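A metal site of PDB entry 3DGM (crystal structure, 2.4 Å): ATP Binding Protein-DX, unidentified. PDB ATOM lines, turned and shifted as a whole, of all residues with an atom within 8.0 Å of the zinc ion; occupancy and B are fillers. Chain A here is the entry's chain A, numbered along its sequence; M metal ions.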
ATOM      1  N   PRO A  24      21.006  10.121 -22.509  1.00  0.00           N
ATOM      2  CA  PRO A  24      20.991  11.588 -22.628  1.00  0.00           C
ATOM      3  C   PRO A  24      19.651  12.145 -22.129  1.00  0.00           C
ATOM      4  O   PRO A  24      18.722  11.378 -21.775  1.00  0.00           O
ATOM      5  CB  PRO A  24      21.152  11.832 -24.153  1.00  0.00           C
ATOM      6  CG  PRO A  24      20.600  10.562 -24.810  1.00  0.00           C
ATOM      7  CD  PRO A  24      20.883   9.456 -23.829  1.00  0.00           C
ATOM      8  N   CYS A  25      19.550  13.473 -22.080  1.00  0.00           N
ATOM      9  CA  CYS A  25      18.314  14.202 -21.722  1.00  0.00           C
ATOM     10  C   CYS A  25      17.061  13.526 -22.323  1.00  0.00           C
ATOM     11  O   CYS A  25      17.059  13.219 -23.516  1.00  0.00           O
ATOM     12  CB  CYS A  25      18.447  15.634 -22.250  1.00  0.00           C
ATOM     13  SG  CYS A  25      16.990  16.640 -21.944  1.00  0.00           S
ATOM     14  N   VAL A  26      16.009  13.303 -21.517  1.00  0.00           N
ATOM     15  CA  VAL A  26      14.770  12.680 -22.057  1.00  0.00           C
ATOM     16  C   VAL A  26      14.011  13.566 -23.067  1.00  0.00           C
ATOM     17  O   VAL A  26      13.100  13.081 -23.749  1.00  0.00           O
ATOM     18  CB  VAL A  26      13.731  12.286 -20.946  1.00  0.00           C
ATOM     19  CG1 VAL A  26      14.269  11.172 -20.003  1.00  0.00           C
ATOM     20  CG2 VAL A  26      13.273  13.519 -20.175  1.00  0.00           C
ATOM     21  N   LYS A  27      14.333  14.863 -23.128  1.00  0.00           N
ATOM     22  CA  LYS A  27      13.582  15.839 -23.933  1.00  0.00           C
ATOM     23  C   LYS A  27      14.331  16.140 -25.233  1.00  0.00           C
ATOM     24  O   LYS A  27      13.775  15.986 -26.308  1.00  0.00           O
ATOM     25  CB  LYS A  27      13.337  17.161 -23.142  1.00  0.00           C
ATOM     26  CG  LYS A  27      12.582  18.264 -23.902  1.00  0.00           C
ATOM     27  CD  LYS A  27      11.144  17.750 -24.274  1.00  0.00           C
ATOM     28  CE  LYS A  27      10.367  18.702 -25.114  1.00  0.00           C
ATOM     29  NZ  LYS A  27       8.966  18.238 -25.252  1.00  0.00           N
ATOM     30  N   CYS A  28      15.584  16.553 -25.157  1.00  0.00           N
ATOM     31  CA  CYS A  28      16.317  16.817 -26.410  1.00  0.00           C
ATOM     32  C   CYS A  28      17.017  15.574 -26.925  1.00  0.00           C
ATOM     33  O   CYS A  28      17.413  15.518 -28.098  1.00  0.00           O
ATOM     34  CB  CYS A  28      17.304  17.979 -26.288  1.00  0.00           C
ATOM     35  SG  CYS A  28      18.762  17.628 -25.193  1.00  0.00           S
ATOM     36  N   LYS A  29      17.195  14.576 -26.059  1.00  0.00           N
ATOM     37  CA  LYS A  29      17.836  13.291 -26.429  1.00  0.00           C
ATOM     38  C   LYS A  29      19.309  13.414 -26.859  1.00  0.00           C
ATOM     39  O   LYS A  29      19.847  12.450 -27.326  1.00  0.00           O
ATOM     40  CB  LYS A  29      17.131  12.545 -27.589  1.00  0.00           C
ATOM     41  CG  LYS A  29      15.633  12.736 -27.797  1.00  0.00           C
ATOM     42  CD  LYS A  29      14.800  11.855 -26.866  1.00  0.00           C
ATOM     43  CE  LYS A  29      13.409  11.744 -27.453  1.00  0.00           C
ATOM     44  NZ  LYS A  29      12.603  10.746 -26.713  1.00  0.00           N
ATOM     45  N   VAL A  30      19.918  14.569 -26.713  1.00  0.00           N
ATOM     46  CA  VAL A  30      21.304  14.786 -27.118  1.00  0.00           C
ATOM     47  C   VAL A  30      22.217  15.142 -25.909  1.00  0.00           C
ATOM     48  O   VAL A  30      23.188  14.402 -25.588  1.00  0.00           O
ATOM     49  CB  VAL A  30      21.358  15.859 -28.242  1.00  0.00           C
ATOM     50  CG1 VAL A  30      22.783  16.281 -28.519  1.00  0.00           C
ATOM     51  CG2 VAL A  30      20.688  15.292 -29.501  1.00  0.00           C
ATOM     52  N   ALA A  31      21.893  16.249 -25.211  1.00  0.00           N
ATOM     53  CA  ALA A  31      22.684  16.729 -24.079  1.00  0.00           C
ATOM     54  C   ALA A  31      22.673  15.735 -22.915  1.00  0.00           C
ATOM     55  O   ALA A  31      21.684  15.043 -22.668  1.00  0.00           O
ATOM     56  CB  ALA A  31      22.212  18.099 -23.635  1.00  0.00           C
ATOM     57  N   PRO A  32      23.783  15.653 -22.198  1.00  0.00           N
ATOM     58  CA  PRO A  32      23.764  14.878 -20.968  1.00  0.00           C
ATOM     59  C   PRO A  32      22.758  15.461 -19.959  1.00  0.00           C
ATOM     60  O   PRO A  32      22.414  16.622 -20.025  1.00  0.00           O
ATOM     61  CB  PRO A  32      25.189  14.996 -20.438  1.00  0.00           C
ATOM     62  CG  PRO A  32      25.980  15.765 -21.475  1.00  0.00           C
ATOM     63  CD  PRO A  32      25.074  16.318 -22.473  1.00  0.00           C
ATOM     64  N   ARG A  33      22.322  14.646 -19.010  1.00  0.00           N
ATOM     65  CA  ARG A  33      21.413  15.101 -17.953  1.00  0.00           C
ATOM     66  C   ARG A  33      22.071  16.005 -16.865  1.00  0.00           C
ATOM     67  O   ARG A  33      23.254  15.852 -16.517  1.00  0.00           O
ATOM     68  CB  ARG A  33      20.765  13.882 -17.304  1.00  0.00           C
ATOM     69  CG  ARG A  33      19.749  13.204 -18.186  1.00  0.00           C
ATOM     70  CD  ARG A  33      19.299  11.886 -17.603  1.00  0.00           C
ATOM     71  NE  ARG A  33      18.728  11.107 -18.691  1.00  0.00           N
ATOM     72  CZ  ARG A  33      17.806  10.156 -18.563  1.00  0.00           C
ATOM     73  NH1 ARG A  33      17.296   9.825 -17.378  1.00  0.00           N
ATOM     74  NH2 ARG A  33      17.363   9.548 -19.663  1.00  0.00           N
ATOM     75  N   ASP A  34      21.285  16.938 -16.323  1.00  0.00           N
ATOM     76  CA  ASP A  34      21.665  17.605 -15.091  1.00  0.00           C
ATOM     77  C   ASP A  34      21.678  16.587 -13.959  1.00  0.00           C
ATOM     78  O   ASP A  34      21.053  15.518 -14.078  1.00  0.00           O
ATOM     79  CB  ASP A  34      20.717  18.785 -14.749  1.00  0.00           C
ATOM     80  CG  ASP A  34      21.297  19.706 -13.671  1.00  0.00           C
ATOM     81  OD1 ASP A  34      22.552  19.757 -13.485  1.00  0.00           O
ATOM     82  OD2 ASP A  34      20.506  20.398 -13.011  1.00  0.00           O
ATOM     83  N   ASN A  46      16.068  13.922 -15.083  1.00  0.00           N
ATOM     84  CA  ASN A  46      15.695  13.451 -16.419  1.00  0.00           C
ATOM     85  C   ASN A  46      16.165  14.327 -17.577  1.00  0.00           C
ATOM     86  O   ASN A  46      16.345  13.817 -18.682  1.00  0.00           O
ATOM     87  CB  ASN A  46      14.179  13.233 -16.500  1.00  0.00           C
ATOM     88  CG  ASN A  46      13.655  12.267 -15.428  1.00  0.00           C
ATOM     89  OD1 ASN A  46      14.422  11.421 -14.900  1.00  0.00           O
ATOM     90  ND2 ASN A  46      12.353  12.351 -15.138  1.00  0.00           N
ATOM     91  N   MET A  47      16.319  15.631 -17.341  1.00  0.00           N
ATOM     92  CA  MET A  47      16.644  16.585 -18.407  1.00  0.00           C
ATOM     93  C   MET A  47      17.988  17.281 -18.205  1.00  0.00           C
ATOM     94  O   MET A  47      18.481  17.376 -17.065  1.00  0.00           O
ATOM     95  CB  MET A  47      15.550  17.654 -18.584  1.00  0.00           C
ATOM     96  CG  MET A  47      14.300  17.116 -19.262  1.00  0.00           C
ATOM     97  SD  MET A  47      12.982  18.308 -19.523  1.00  0.00           S
ATOM     98  CE  MET A  47      12.516  18.704 -17.796  1.00  0.00           C
ATOM     99  N   CYS A  48      18.581  17.735 -19.320  1.00  0.00           N
ATOM    100  CA  CYS A  48      19.685  18.669 -19.205  1.00  0.00           C
ATOM    101  C   CYS A  48      19.134  20.013 -18.604  1.00  0.00           C
ATOM    102  O   CYS A  48      17.897  20.195 -18.457  1.00  0.00           O
ATOM    103  CB  CYS A  48      20.399  18.876 -20.542  1.00  0.00           C
ATOM    104  SG  CYS A  48      19.418  19.747 -21.769  1.00  0.00           S
ATOM    105  N   LYS A  49      20.016  20.928 -18.242  1.00  0.00           N
ATOM    106  CA  LYS A  49      19.556  22.116 -17.580  1.00  0.00           C
ATOM    107  C   LYS A  49      18.770  22.990 -18.568  1.00  0.00           C
ATOM    108  O   LYS A  49      17.717  23.533 -18.208  1.00  0.00           O
ATOM    109  CB  LYS A  49      20.702  22.926 -16.979  1.00  0.00           C
ATOM    110  CG  LYS A  49      20.219  24.042 -16.070  1.00  0.00           C
ATOM    111  CD  LYS A  49      20.062  23.517 -14.635  1.00  0.00           C
ATOM    112  CE  LYS A  49      18.977  24.257 -13.924  1.00  0.00           C
ATOM    113  NZ  LYS A  49      19.008  23.789 -12.511  1.00  0.00           N
ATOM    114  N   THR A  50      19.254  23.098 -19.807  1.00  0.00           N
ATOM    115  CA  THR A  50      18.634  23.939 -20.816  1.00  0.00           C
ATOM    116  C   THR A  50      17.188  23.504 -21.015  1.00  0.00           C
ATOM    117  O   THR A  50      16.289  24.361 -21.079  1.00  0.00           O
ATOM    118  CB  THR A  50      19.348  23.797 -22.166  1.00  0.00           C
ATOM    119  OG1 THR A  50      20.725  24.178 -22.020  1.00  0.00           O
ATOM    120  CG2 THR A  50      18.678  24.683 -23.251  1.00  0.00           C
ATOM    121  N   CYS A  51      16.961  22.175 -21.121  1.00  0.00           N
ATOM    122  CA  CYS A  51      15.592  21.646 -21.347  1.00  0.00           C
ATOM    123  C   CYS A  51      14.749  21.801 -20.106  1.00  0.00           C
ATOM    124  O   CYS A  51      13.559  22.145 -20.221  1.00  0.00           O
ATOM    125  CB  CYS A  51      15.578  20.184 -21.793  1.00  0.00           C
ATOM    126  SG  CYS A  51      16.108  19.963 -23.475  1.00  0.00           S
ATOM    127  N   PHE A  52      15.340  21.584 -18.934  1.00  0.00           N
ATOM    128  CA  PHE A  52      14.638  21.842 -17.666  1.00  0.00           C
ATOM    129  C   PHE A  52      14.116  23.279 -17.515  1.00  0.00           C
ATOM    130  O   PHE A  52      12.912  23.510 -17.258  1.00  0.00           O
ATOM    131  CB  PHE A  52      15.487  21.506 -16.424  1.00  0.00           C
ATOM    132  CG  PHE A  52      14.752  21.753 -15.150  1.00  0.00           C
ATOM    133  CD1 PHE A  52      13.560  21.034 -14.883  1.00  0.00           C
ATOM    134  CD2 PHE A  52      15.166  22.751 -14.260  1.00  0.00           C
ATOM    135  CE1 PHE A  52      12.813  21.266 -13.706  1.00  0.00           C
ATOM    136  CE2 PHE A  52      14.428  23.023 -13.051  1.00  0.00           C
ATOM    137  CZ  PHE A  52      13.262  22.272 -12.779  1.00  0.00           C
HETATM  138 ZN    ZN M   1      17.844  18.504 -23.110  1.00  0.00          ZN
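Four residues have an atom within 4 Å of the zinc ion: Cys 25, Cys 28, Cys 48 and Cys 51.
The zinc ion is bound by the side-chain sulfur of Cys 51, the side-chain sulfur of Cys 25, the side-chain sulfur of Cys 48 and the side-chain sulfur of Cys 28.
The zinc ion has four donor atoms within binding distance.
O of Ala 31 lies within hydrogen-bond range of N of Cys 25, 2.7 Å away.
N of Val 30 sits close to SG of Cys 28, 3.6 Å away.
The side-chain sulfur of Cys 28 sits close to the backbone NH of Ala 31 (3.4 Å).
The side-chain sulfur of Cys 25 sits close to the backbone NH of Lys 27, 3.4 Å away.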
